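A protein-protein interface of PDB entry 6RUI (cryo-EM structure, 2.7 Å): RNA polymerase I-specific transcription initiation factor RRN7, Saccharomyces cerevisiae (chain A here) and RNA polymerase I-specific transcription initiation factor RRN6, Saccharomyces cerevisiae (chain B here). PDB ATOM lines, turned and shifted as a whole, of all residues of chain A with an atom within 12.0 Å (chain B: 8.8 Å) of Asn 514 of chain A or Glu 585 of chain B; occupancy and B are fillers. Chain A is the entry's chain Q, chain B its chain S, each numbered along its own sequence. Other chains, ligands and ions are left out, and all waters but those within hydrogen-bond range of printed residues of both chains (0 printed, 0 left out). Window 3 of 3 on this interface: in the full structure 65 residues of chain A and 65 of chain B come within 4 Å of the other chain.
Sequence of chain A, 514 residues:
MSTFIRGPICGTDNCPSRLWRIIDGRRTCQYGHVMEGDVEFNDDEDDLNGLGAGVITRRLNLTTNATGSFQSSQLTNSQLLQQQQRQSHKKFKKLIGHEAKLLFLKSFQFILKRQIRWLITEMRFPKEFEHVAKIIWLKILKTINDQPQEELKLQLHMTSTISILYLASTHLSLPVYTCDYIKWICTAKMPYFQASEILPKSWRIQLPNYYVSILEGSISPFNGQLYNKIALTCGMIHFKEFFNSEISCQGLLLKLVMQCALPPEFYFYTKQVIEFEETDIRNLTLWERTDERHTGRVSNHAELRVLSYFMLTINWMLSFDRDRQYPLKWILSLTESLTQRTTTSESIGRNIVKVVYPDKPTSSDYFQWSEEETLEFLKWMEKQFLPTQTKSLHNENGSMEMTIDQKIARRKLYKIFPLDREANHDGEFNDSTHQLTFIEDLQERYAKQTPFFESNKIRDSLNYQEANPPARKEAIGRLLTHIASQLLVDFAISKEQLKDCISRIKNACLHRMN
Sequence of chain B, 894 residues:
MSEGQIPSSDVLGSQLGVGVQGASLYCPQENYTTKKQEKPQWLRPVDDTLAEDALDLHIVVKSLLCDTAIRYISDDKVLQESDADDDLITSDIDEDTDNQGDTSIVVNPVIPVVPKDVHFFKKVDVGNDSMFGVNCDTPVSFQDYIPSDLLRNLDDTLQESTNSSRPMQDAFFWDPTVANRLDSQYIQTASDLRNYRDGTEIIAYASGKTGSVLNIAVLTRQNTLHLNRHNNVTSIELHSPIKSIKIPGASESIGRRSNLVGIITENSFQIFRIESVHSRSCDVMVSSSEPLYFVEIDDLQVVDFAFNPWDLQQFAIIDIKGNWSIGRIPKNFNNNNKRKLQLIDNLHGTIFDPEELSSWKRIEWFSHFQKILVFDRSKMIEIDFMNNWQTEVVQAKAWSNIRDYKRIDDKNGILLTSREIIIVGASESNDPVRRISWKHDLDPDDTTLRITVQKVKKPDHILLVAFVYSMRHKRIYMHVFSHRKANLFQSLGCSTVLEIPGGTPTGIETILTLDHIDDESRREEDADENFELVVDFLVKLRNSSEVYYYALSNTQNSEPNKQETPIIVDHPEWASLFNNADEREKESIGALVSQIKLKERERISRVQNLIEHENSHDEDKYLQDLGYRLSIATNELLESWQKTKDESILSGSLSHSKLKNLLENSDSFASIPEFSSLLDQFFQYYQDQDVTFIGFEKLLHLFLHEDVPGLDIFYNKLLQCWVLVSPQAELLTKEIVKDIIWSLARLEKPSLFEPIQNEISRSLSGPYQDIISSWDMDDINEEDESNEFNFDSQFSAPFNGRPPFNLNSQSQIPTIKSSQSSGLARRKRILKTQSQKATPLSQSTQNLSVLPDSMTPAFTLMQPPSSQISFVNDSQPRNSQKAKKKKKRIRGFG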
ATOM      1  N   PHE A 276      -9.467  -3.389  18.238  1.00  0.00           N
ATOM      2  CA  PHE A 276      -8.527  -3.607  19.331  1.00  0.00           C
ATOM      3  C   PHE A 276      -8.118  -2.291  19.983  1.00  0.00           C
ATOM      4  O   PHE A 276      -7.946  -2.222  21.204  1.00  0.00           O
ATOM      5  CB  PHE A 276      -7.303  -4.350  18.797  1.00  0.00           C
ATOM      6  CG  PHE A 276      -6.322  -4.746  19.851  1.00  0.00           C
ATOM      7  CD1 PHE A 276      -6.563  -5.846  20.653  1.00  0.00           C
ATOM      8  CD2 PHE A 276      -5.151  -4.026  20.034  1.00  0.00           C
ATOM      9  CE1 PHE A 276      -5.661  -6.222  21.621  1.00  0.00           C
ATOM     10  CE2 PHE A 276      -4.250  -4.395  21.002  1.00  0.00           C
ATOM     11  CZ  PHE A 276      -4.504  -5.496  21.796  1.00  0.00           C
ATOM     12  N   GLU A 277      -7.953  -1.238  19.180  1.00  0.00           N
ATOM     13  CA  GLU A 277      -7.474   0.067  19.637  1.00  0.00           C
ATOM     14  C   GLU A 277      -8.394   1.146  19.059  1.00  0.00           C
ATOM     15  O   GLU A 277      -8.078   1.730  18.019  1.00  0.00           O
ATOM     16  CB  GLU A 277      -6.009   0.256  19.201  1.00  0.00           C
ATOM     17  CG  GLU A 277      -5.307   1.532  19.658  1.00  0.00           C
ATOM     18  CD  GLU A 277      -5.008   1.535  21.128  1.00  0.00           C
ATOM     19  OE1 GLU A 277      -4.849   0.439  21.689  1.00  0.00           O
ATOM     20  OE2 GLU A 277      -4.931   2.628  21.723  1.00  0.00           O
ATOM     21  N   LEU A 312      -0.010  -1.032   9.188  1.00  0.00           N
ATOM     22  CA  LEU A 312       0.502  -2.022  10.126  1.00  0.00           C
ATOM     23  C   LEU A 312      -0.182  -3.368   9.991  1.00  0.00           C
ATOM     24  O   LEU A 312       0.436  -4.396  10.267  1.00  0.00           O
ATOM     25  CB  LEU A 312       0.355  -1.515  11.568  1.00  0.00           C
ATOM     26  CG  LEU A 312       1.438  -0.602  12.163  1.00  0.00           C
ATOM     27  CD1 LEU A 312       1.454   0.796  11.570  1.00  0.00           C
ATOM     28  CD2 LEU A 312       1.266  -0.505  13.663  1.00  0.00           C
ATOM     29  N   ASN A 315       1.534  -5.435   7.629  1.00  0.00           N
ATOM     30  CA  ASN A 315       2.867  -5.800   8.087  1.00  0.00           C
ATOM     31  C   ASN A 315       2.842  -6.691   9.319  1.00  0.00           C
ATOM     32  O   ASN A 315       3.782  -7.461   9.530  1.00  0.00           O
ATOM     33  CB  ASN A 315       3.683  -4.537   8.395  1.00  0.00           C
ATOM     34  CG  ASN A 315       5.177  -4.788   8.409  1.00  0.00           C
ATOM     35  OD1 ASN A 315       5.634  -5.883   8.113  1.00  0.00           O
ATOM     36  ND2 ASN A 315       5.944  -3.767   8.757  1.00  0.00           N
ATOM     37  N   TRP A 316       1.789  -6.600  10.138  1.00  0.00           N
ATOM     38  CA  TRP A 316       1.616  -7.551  11.230  1.00  0.00           C
ATOM     39  C   TRP A 316       1.424  -8.964  10.701  1.00  0.00           C
ATOM     40  O   TRP A 316       1.996  -9.913  11.245  1.00  0.00           O
ATOM     41  CB  TRP A 316       0.430  -7.145  12.102  1.00  0.00           C
ATOM     42  CG  TRP A 316       0.686  -5.956  12.980  1.00  0.00           C
ATOM     43  CD1 TRP A 316       1.878  -5.333  13.194  1.00  0.00           C
ATOM     44  CD2 TRP A 316      -0.278  -5.258  13.773  1.00  0.00           C
ATOM     45  NE1 TRP A 316       1.716  -4.287  14.067  1.00  0.00           N
ATOM     46  CE2 TRP A 316       0.400  -4.218  14.436  1.00  0.00           C
ATOM     47  CE3 TRP A 316      -1.649  -5.409  13.983  1.00  0.00           C
ATOM     48  CZ2 TRP A 316      -0.248  -3.332  15.297  1.00  0.00           C
ATOM     49  CZ3 TRP A 316      -2.291  -4.533  14.836  1.00  0.00           C
ATOM     50  CH2 TRP A 316      -1.590  -3.503  15.479  1.00  0.00           C
ATOM     51  N   SER A 319       4.952 -10.210   8.304  1.00  0.00           N
ATOM     52  CA  SER A 319       6.271 -10.345   8.913  1.00  0.00           C
ATOM     53  C   SER A 319       6.371 -11.617   9.746  1.00  0.00           C
ATOM     54  O   SER A 319       7.428 -12.254   9.785  1.00  0.00           O
ATOM     55  CB  SER A 319       6.593  -9.118   9.767  1.00  0.00           C
ATOM     56  OG  SER A 319       7.879  -9.218  10.349  1.00  0.00           O
ATOM     57  N   PHE A 320       5.290 -11.992  10.416  1.00  0.00           N
ATOM     58  CA  PHE A 320       5.239 -13.218  11.208  1.00  0.00           C
ATOM     59  C   PHE A 320       4.529 -14.327  10.435  1.00  0.00           C
ATOM     60  O   PHE A 320       3.429 -14.755  10.774  1.00  0.00           O
ATOM     61  CB  PHE A 320       4.571 -12.942  12.549  1.00  0.00           C
ATOM     62  CG  PHE A 320       5.365 -12.021  13.420  1.00  0.00           C
ATOM     63  CD1 PHE A 320       6.408 -12.506  14.196  1.00  0.00           C
ATOM     64  CD2 PHE A 320       5.103 -10.664  13.428  1.00  0.00           C
ATOM     65  CE1 PHE A 320       7.155 -11.653  14.985  1.00  0.00           C
ATOM     66  CE2 PHE A 320       5.844  -9.810  14.208  1.00  0.00           C
ATOM     67  CZ  PHE A 320       6.869 -10.300  14.988  1.00  0.00           C
ATOM     68  N   ARG A 322       3.432 -17.343   9.766  1.00  0.00           N
ATOM     69  CA  ARG A 322       3.258 -18.560  10.548  1.00  0.00           C
ATOM     70  C   ARG A 322       2.629 -19.679   9.731  1.00  0.00           C
ATOM     71  O   ARG A 322       3.077 -20.827   9.800  1.00  0.00           O
ATOM     72  CB  ARG A 322       2.397 -18.248  11.776  1.00  0.00           C
ATOM     73  CG  ARG A 322       2.184 -19.396  12.744  1.00  0.00           C
ATOM     74  CD  ARG A 322       3.494 -19.786  13.386  1.00  0.00           C
ATOM     75  NE  ARG A 322       4.087 -18.673  14.121  1.00  0.00           N
ATOM     76  CZ  ARG A 322       5.357 -18.634  14.511  1.00  0.00           C
ATOM     77  NH1 ARG A 322       6.168 -19.647  14.235  1.00  0.00           N
ATOM     78  NH2 ARG A 322       5.821 -17.583  15.169  1.00  0.00           N
ATOM     79  N   ILE A 505       0.170   5.363  16.854  1.00  0.00           N
ATOM     80  CA  ILE A 505      -0.745   4.237  16.782  1.00  0.00           C
ATOM     81  C   ILE A 505      -0.068   2.947  17.223  1.00  0.00           C
ATOM     82  O   ILE A 505      -0.666   2.142  17.943  1.00  0.00           O
ATOM     83  CB  ILE A 505      -1.337   4.101  15.360  1.00  0.00           C
ATOM     84  CG1 ILE A 505      -2.129   5.356  14.997  1.00  0.00           C
ATOM     85  CG2 ILE A 505      -2.226   2.877  15.226  1.00  0.00           C
ATOM     86  CD1 ILE A 505      -3.291   5.640  15.912  1.00  0.00           C
ATOM     87  N   LYS A 506       1.194   2.755  16.834  1.00  0.00           N
ATOM     88  CA  LYS A 506       1.944   1.591  17.292  1.00  0.00           C
ATOM     89  C   LYS A 506       2.209   1.669  18.788  1.00  0.00           C
ATOM     90  O   LYS A 506       1.986   0.698  19.519  1.00  0.00           O
ATOM     91  CB  LYS A 506       3.256   1.470  16.525  1.00  0.00           C
ATOM     92  CG  LYS A 506       4.072   0.254  16.900  1.00  0.00           C
ATOM     93  CD  LYS A 506       5.339   0.210  16.087  1.00  0.00           C
ATOM     94  CE  LYS A 506       6.191  -0.975  16.464  1.00  0.00           C
ATOM     95  NZ  LYS A 506       7.458  -0.981  15.685  1.00  0.00           N
ATOM     96  N   ASN A 507       2.626   2.833  19.274  1.00  0.00           N
ATOM     97  CA  ASN A 507       2.820   3.007  20.712  1.00  0.00           C
ATOM     98  C   ASN A 507       1.554   3.517  21.395  1.00  0.00           C
ATOM     99  O   ASN A 507       1.543   4.468  22.172  1.00  0.00           O
ATOM    100  CB  ASN A 507       4.008   3.926  20.957  1.00  0.00           C
ATOM    101  CG  ASN A 507       5.317   3.292  20.529  1.00  0.00           C
ATOM    102  OD1 ASN A 507       5.952   3.729  19.568  1.00  0.00           O
ATOM    103  ND2 ASN A 507       5.725   2.247  21.242  1.00  0.00           N
ATOM    104  N   ALA A 508       0.459   2.842  21.062  1.00  0.00           N
ATOM    105  CA  ALA A 508      -0.763   2.763  21.840  1.00  0.00           C
ATOM    106  C   ALA A 508      -1.322   1.356  21.803  1.00  0.00           C
ATOM    107  O   ALA A 508      -2.208   1.038  22.599  1.00  0.00           O
ATOM    108  CB  ALA A 508      -1.820   3.745  21.320  1.00  0.00           C
ATOM    109  N   CYS A 509      -0.823   0.506  20.903  1.00  0.00           N
ATOM    110  CA  CYS A 509      -1.229  -0.884  20.780  1.00  0.00           C
ATOM    111  C   CYS A 509      -0.378  -1.806  21.637  1.00  0.00           C
ATOM    112  O   CYS A 509      -0.898  -2.786  22.178  1.00  0.00           O
ATOM    113  CB  CYS A 509      -1.150  -1.314  19.313  1.00  0.00           C
ATOM    114  SG  CYS A 509      -1.772  -2.970  18.963  1.00  0.00           S
ATOM    115  N   LEU A 510       0.916  -1.508  21.776  1.00  0.00           N
ATOM    116  CA  LEU A 510       1.758  -2.160  22.776  1.00  0.00           C
ATOM    117  C   LEU A 510       1.302  -1.853  24.191  1.00  0.00           C
ATOM    118  O   LEU A 510       1.475  -2.692  25.082  1.00  0.00           O
ATOM    119  CB  LEU A 510       3.216  -1.725  22.621  1.00  0.00           C
ATOM    120  CG  LEU A 510       4.116  -2.428  21.601  1.00  0.00           C
ATOM    121  CD1 LEU A 510       3.795  -2.045  20.159  1.00  0.00           C
ATOM    122  CD2 LEU A 510       5.590  -2.175  21.917  1.00  0.00           C
ATOM    123  N   HIS A 511       0.690  -0.684  24.399  1.00  0.00           N
ATOM    124  CA  HIS A 511       0.135  -0.282  25.682  1.00  0.00           C
ATOM    125  C   HIS A 511      -1.049  -1.149  26.099  1.00  0.00           C
ATOM    126  O   HIS A 511      -1.427  -1.136  27.274  1.00  0.00           O
ATOM    127  CB  HIS A 511      -0.257   1.193  25.585  1.00  0.00           C
ATOM    128  CG  HIS A 511      -0.667   1.816  26.881  1.00  0.00           C
ATOM    129  ND1 HIS A 511      -1.960   1.762  27.356  1.00  0.00           N
ATOM    130  CD2 HIS A 511       0.037   2.535  27.788  1.00  0.00           C
ATOM    131  CE1 HIS A 511      -2.032   2.408  28.506  1.00  0.00           C
ATOM    132  NE2 HIS A 511      -0.834   2.884  28.792  1.00  0.00           N
ATOM    133  N   ARG A 512      -1.636  -1.911  25.173  1.00  0.00           N
ATOM    134  CA  ARG A 512      -2.694  -2.846  25.538  1.00  0.00           C
ATOM    135  C   ARG A 512      -2.133  -4.156  26.072  1.00  0.00           C
ATOM    136  O   ARG A 512      -2.694  -4.734  27.011  1.00  0.00           O
ATOM    137  CB  ARG A 512      -3.599  -3.112  24.343  1.00  0.00           C
ATOM    138  CG  ARG A 512      -4.306  -1.880  23.870  1.00  0.00           C
ATOM    139  CD  ARG A 512      -5.297  -1.388  24.906  1.00  0.00           C
ATOM    140  NE  ARG A 512      -6.397  -2.327  25.101  1.00  0.00           N
ATOM    141  CZ  ARG A 512      -7.531  -2.299  24.409  1.00  0.00           C
ATOM    142  NH1 ARG A 512      -7.724  -1.370  23.482  1.00  0.00           N
ATOM    143  NH2 ARG A 512      -8.476  -3.193  24.649  1.00  0.00           N
ATOM    144  N   MET A 513      -1.040  -4.648  25.488  1.00  0.00           N
ATOM    145  CA  MET A 513      -0.478  -5.917  25.936  1.00  0.00           C
ATOM    146  C   MET A 513       0.258  -5.763  27.262  1.00  0.00           C
ATOM    147  O   MET A 513      -0.075  -6.426  28.250  1.00  0.00           O
ATOM    148  CB  MET A 513       0.443  -6.496  24.867  1.00  0.00           C
ATOM    149  CG  MET A 513      -0.279  -7.144  23.700  1.00  0.00           C
ATOM    150  SD  MET A 513      -1.021  -5.973  22.559  1.00  0.00           S
ATOM    151  CE  MET A 513      -1.295  -7.041  21.150  1.00  0.00           C
ATOM    152  N   ASN A 514       1.266  -4.901  27.308  1.00  0.00           N
ATOM    153  CA  ASN A 514       1.968  -4.672  28.566  1.00  0.00           C
ATOM    154  C   ASN A 514       1.934  -3.208  29.003  1.00  0.00           C
ATOM    155  O   ASN A 514       0.897  -2.710  29.436  1.00  0.00           O
ATOM    156  CB  ASN A 514       3.417  -5.179  28.479  1.00  0.00           C
ATOM    157  CG  ASN A 514       4.213  -4.547  27.344  1.00  0.00           C
ATOM    158  OD1 ASN A 514       3.728  -3.693  26.605  1.00  0.00           O
ATOM    159  ND2 ASN A 514       5.460  -4.965  27.219  1.00  0.00           N
ATOM    160  N   ASN B 580      10.798  -4.677  16.369  1.00  0.00           N
ATOM    161  CA  ASN B 580      11.472  -4.505  17.646  1.00  0.00           C
ATOM    162  C   ASN B 580      12.229  -5.774  18.038  1.00  0.00           C
ATOM    163  O   ASN B 580      11.885  -6.888  17.640  1.00  0.00           O
ATOM    164  CB  ASN B 580      10.464  -4.135  18.741  1.00  0.00           C
ATOM    165  CG  ASN B 580       9.770  -2.802  18.483  1.00  0.00           C
ATOM    166  OD1 ASN B 580       8.561  -2.751  18.267  1.00  0.00           O
ATOM    167  ND2 ASN B 580      10.533  -1.718  18.525  1.00  0.00           N
ATOM    168  N   ALA B 581      13.282  -5.589  18.837  1.00  0.00           N
ATOM    169  CA  ALA B 581      14.130  -6.684  19.298  1.00  0.00           C
ATOM    170  C   ALA B 581      13.660  -7.266  20.622  1.00  0.00           C
ATOM    171  O   ALA B 581      14.459  -7.847  21.367  1.00  0.00           O
ATOM    172  CB  ALA B 581      15.580  -6.215  19.411  1.00  0.00           C
ATOM    173  N   ASP B 582      12.378  -7.133  20.921  1.00  0.00           N
ATOM    174  CA  ASP B 582      11.829  -7.432  22.237  1.00  0.00           C
ATOM    175  C   ASP B 582      11.179  -8.807  22.174  1.00  0.00           C
ATOM    176  O   ASP B 582      10.029  -8.943  21.752  1.00  0.00           O
ATOM    177  CB  ASP B 582      10.840  -6.344  22.627  1.00  0.00           C
ATOM    178  CG  ASP B 582      11.510  -5.009  22.852  1.00  0.00           C
ATOM    179  OD1 ASP B 582      12.679  -5.001  23.292  1.00  0.00           O
ATOM    180  OD2 ASP B 582      10.872  -3.972  22.577  1.00  0.00           O
ATOM    181  N   GLU B 583      11.924  -9.830  22.596  1.00  0.00           N
ATOM    182  CA  GLU B 583      11.502 -11.213  22.415  1.00  0.00           C
ATOM    183  C   GLU B 583      10.344 -11.603  23.323  1.00  0.00           C
ATOM    184  O   GLU B 583       9.582 -12.509  22.976  1.00  0.00           O
ATOM    185  CB  GLU B 583      12.680 -12.162  22.655  1.00  0.00           C
ATOM    186  CG  GLU B 583      13.828 -12.037  21.658  1.00  0.00           C
ATOM    187  CD  GLU B 583      14.836 -10.975  22.057  1.00  0.00           C
ATOM    188  OE1 GLU B 583      14.670 -10.373  23.138  1.00  0.00           O
ATOM    189  OE2 GLU B 583      15.799 -10.742  21.296  1.00  0.00           O
ATOM    190  N   ARG B 584      10.203 -10.951  24.473  1.00  0.00           N
ATOM    191  CA  ARG B 584       9.020 -11.149  25.298  1.00  0.00           C
ATOM    192  C   ARG B 584       7.813 -10.436  24.699  1.00  0.00           C
ATOM    193  O   ARG B 584       6.681 -10.925  24.805  1.00  0.00           O
ATOM    194  CB  ARG B 584       9.313 -10.669  26.724  1.00  0.00           C
ATOM    195  CG  ARG B 584       8.151 -10.753  27.697  1.00  0.00           C
ATOM    196  CD  ARG B 584       7.695 -12.182  27.922  1.00  0.00           C
ATOM    197  NE  ARG B 584       6.564 -12.248  28.842  1.00  0.00           N
ATOM    198  CZ  ARG B 584       5.293 -12.099  28.478  1.00  0.00           C
ATOM    199  NH1 ARG B 584       4.984 -11.873  27.207  1.00  0.00           N
ATOM    200  NH2 ARG B 584       4.327 -12.173  29.382  1.00  0.00           N
ATOM    201  N   GLU B 585       8.044  -9.312  24.034  1.00  0.00           N
ATOM    202  CA  GLU B 585       7.012  -8.582  23.316  1.00  0.00           C
ATOM    203  C   GLU B 585       6.867  -9.057  21.877  1.00  0.00           C
ATOM    204  O   GLU B 585       6.050  -8.510  21.133  1.00  0.00           O
ATOM    205  CB  GLU B 585       7.331  -7.085  23.350  1.00  0.00           C
ATOM    206  CG  GLU B 585       7.180  -6.413  24.712  1.00  0.00           C
ATOM    207  CD  GLU B 585       8.351  -6.640  25.656  1.00  0.00           C
ATOM    208  OE1 GLU B 585       9.314  -7.337  25.285  1.00  0.00           O
ATOM    209  OE2 GLU B 585       8.308  -6.118  26.789  1.00  0.00           O
ATOM    210  N   LYS B 586       7.652 -10.057  21.477  1.00  0.00           N
ATOM    211  CA  LYS B 586       7.613 -10.571  20.112  1.00  0.00           C
ATOM    212  C   LYS B 586       6.322 -11.330  19.849  1.00  0.00           C
ATOM    213  O   LYS B 586       5.552 -10.982  18.945  1.00  0.00           O
ATOM    214  CB  LYS B 586       8.821 -11.472  19.882  1.00  0.00           C
ATOM    215  CG  LYS B 586       8.939 -12.086  18.512  1.00  0.00           C
ATOM    216  CD  LYS B 586      10.164 -12.974  18.495  1.00  0.00           C
ATOM    217  CE  LYS B 586      10.326 -13.704  17.188  1.00  0.00           C
ATOM    218  NZ  LYS B 586      11.521 -14.589  17.242  1.00  0.00           N
ATOM    219  N   GLU B 587       6.070 -12.382  20.628  1.00  0.00           N
ATOM    220  CA  GLU B 587       4.807 -13.091  20.500  1.00  0.00           C
ATOM    221  C   GLU B 587       3.667 -12.354  21.181  1.00  0.00           C
ATOM    222  O   GLU B 587       2.508 -12.654  20.896  1.00  0.00           O
ATOM    223  CB  GLU B 587       4.907 -14.507  21.077  1.00  0.00           C
ATOM    224  CG  GLU B 587       4.923 -14.577  22.600  1.00  0.00           C
ATOM    225  CD  GLU B 587       6.316 -14.532  23.190  1.00  0.00           C
ATOM    226  OE1 GLU B 587       7.272 -14.210  22.453  1.00  0.00           O
ATOM    227  OE2 GLU B 587       6.453 -14.820  24.399  1.00  0.00           O
ATOM    228  N   SER B 588       3.965 -11.411  22.079  1.00  0.00           N
ATOM    229  CA  SER B 588       2.908 -10.606  22.682  1.00  0.00           C
ATOM    230  C   SER B 588       2.292  -9.682  21.644  1.00  0.00           C
ATOM    231  O   SER B 588       1.086  -9.416  21.662  1.00  0.00           O
ATOM    232  CB  SER B 588       3.465  -9.813  23.862  1.00  0.00           C
ATOM    233  OG  SER B 588       2.452  -9.065  24.503  1.00  0.00           O
ATOM    234  N   ILE B 589       3.117  -9.184  20.724  1.00  0.00           N
ATOM    235  CA  ILE B 589       2.603  -8.630  19.480  1.00  0.00           C
ATOM    236  C   ILE B 589       2.083  -9.745  18.581  1.00  0.00           C
ATOM    237  O   ILE B 589       0.974  -9.665  18.039  1.00  0.00           O
ATOM    238  CB  ILE B 589       3.694  -7.796  18.782  1.00  0.00           C
ATOM    239  CG1 ILE B 589       3.975  -6.516  19.568  1.00  0.00           C
ATOM    240  CG2 ILE B 589       3.315  -7.476  17.348  1.00  0.00           C
ATOM    241  CD1 ILE B 589       5.197  -5.769  19.089  1.00  0.00           C
ATOM    242  N   GLY B 590       2.857 -10.825  18.453  1.00  0.00           N
ATOM    243  CA  GLY B 590       2.533 -11.918  17.552  1.00  0.00           C
ATOM    244  C   GLY B 590       1.343 -12.765  17.961  1.00  0.00           C
ATOM    245  O   GLY B 590       0.926 -13.625  17.176  1.00  0.00           O
ATOM    246  N   ALA B 591       0.800 -12.559  19.167  1.00  0.00           N
ATOM    247  CA  ALA B 591      -0.439 -13.233  19.540  1.00  0.00           C
ATOM    248  C   ALA B 591      -1.614 -12.709  18.736  1.00  0.00           C
ATOM    249  O   ALA B 591      -2.543 -13.464  18.439  1.00  0.00           O
ATOM    250  CB  ALA B 591      -0.717 -13.065  21.033  1.00  0.00           C
ATOM    251  N   LEU B 592      -1.573 -11.430  18.366  1.00  0.00           N
ATOM    252  CA  LEU B 592      -2.687 -10.808  17.666  1.00  0.00           C
ATOM    253  C   LEU B 592      -2.817 -11.340  16.248  1.00  0.00           C
ATOM    254  O   LEU B 592      -3.925 -11.396  15.704  1.00  0.00           O
ATOM    255  CB  LEU B 592      -2.499  -9.290  17.680  1.00  0.00           C
ATOM    256  CG  LEU B 592      -3.612  -8.343  17.241  1.00  0.00           C
ATOM    257  CD1 LEU B 592      -3.539  -7.085  18.082  1.00  0.00           C
ATOM    258  CD2 LEU B 592      -3.488  -7.980  15.767  1.00  0.00           C
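Of the 18 printed residues of chain A, 6 touch a printed residue of chain B. Hydrophobic or aromatic side chains of chain A that line the printed part of chain B: Phe 276, Trp 316, Phe 320 and Met 513. Of the 13 printed residues of chain B, 5 touch a printed residue of chain A. Printed residues of chain B that touch a printed residue of chain A: Asn 580, Glu 585, Lys 586, Ser 588 and Leu 592. Among the printed residues, no Asp or Glu carboxylate lies within 4 Å of a Lys or Arg side-chain nitrogen of the other chain.
CD2 of Phe 276 of chain A touches CD1 of Leu 592 of chain B, at 3.97 Å. Trp 316 of chain A touches Leu 592 of chain B. CE1 of Phe 320 of chain A touches CG of Lys 586 of chain B, at 3.98 Å. Ser 588 of chain B touches Met 513 of chain A (OG to CB, 3.3 Å). Met 513 of chain A touches Leu 592 of chain B (CE to CD1, 3.8 Å).
The side-chain amide nitrogen of Asn 514 of chain A sits at hydrogen-bond distance from the side-chain carboxylate of Glu 585 of chain B (3.1 Å). The side-chain amide oxygen (OD1) of Asn 580 of chain B is in hydrogen-bond range of the side-chain amino group (NZ) of Lys 506 of chain A, at 3.3 Å.
The side-chain amide oxygen (OD1) of Asn 514 of chain A sits close to the backbone carbonyl oxygen (O) of Leu 510 of chain A, at 2.9 Å. The backbone carbonyl oxygen (O) of Phe 276 of chain A is in hydrogen-bond range of the guanidinium group (NH1) of Arg 512 of chain A, at 2.4 Å.
Asn 514 of chain A touches just one residue of chain B: Glu 585. Glu 585 of chain B touches just one residue of chain A: Asn 514. Of chain A, only Lys 506 comes within 4 Å of Asn 580 of chain B. No residue of chain A comes within 4 Å of Arg 584 of chain B. No residue of chain A comes within 4 Å of Glu 587 of chain B. Ser 588 of chain B touches one residue of chain A. Of the printed residues of chain B, Met 513 of chain A touches Ser 588 (3.3 Å) and Leu 592 (3.8 Å). Of the printed residues of chain B, Phe 276 of chain A touches Leu 592. Of the printed residues of chain A, Lys 586 of chain B touches Phe 320. Of the printed residues of chain B, Trp 316 of chain A touches Leu 592 (3.6 Å). The nearest residue of chain B that does not touch Asn 514 of chain A is Ser 588 of chain B (5.2 Å). The nearest residue of chain A that does not touch Glu 585 of chain B is Leu 510 of chain A (5.3 Å). The nearest printed residue of chain B that does not touch Phe 320 of chain A is Ile 589 of chain B (4.7 Å).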
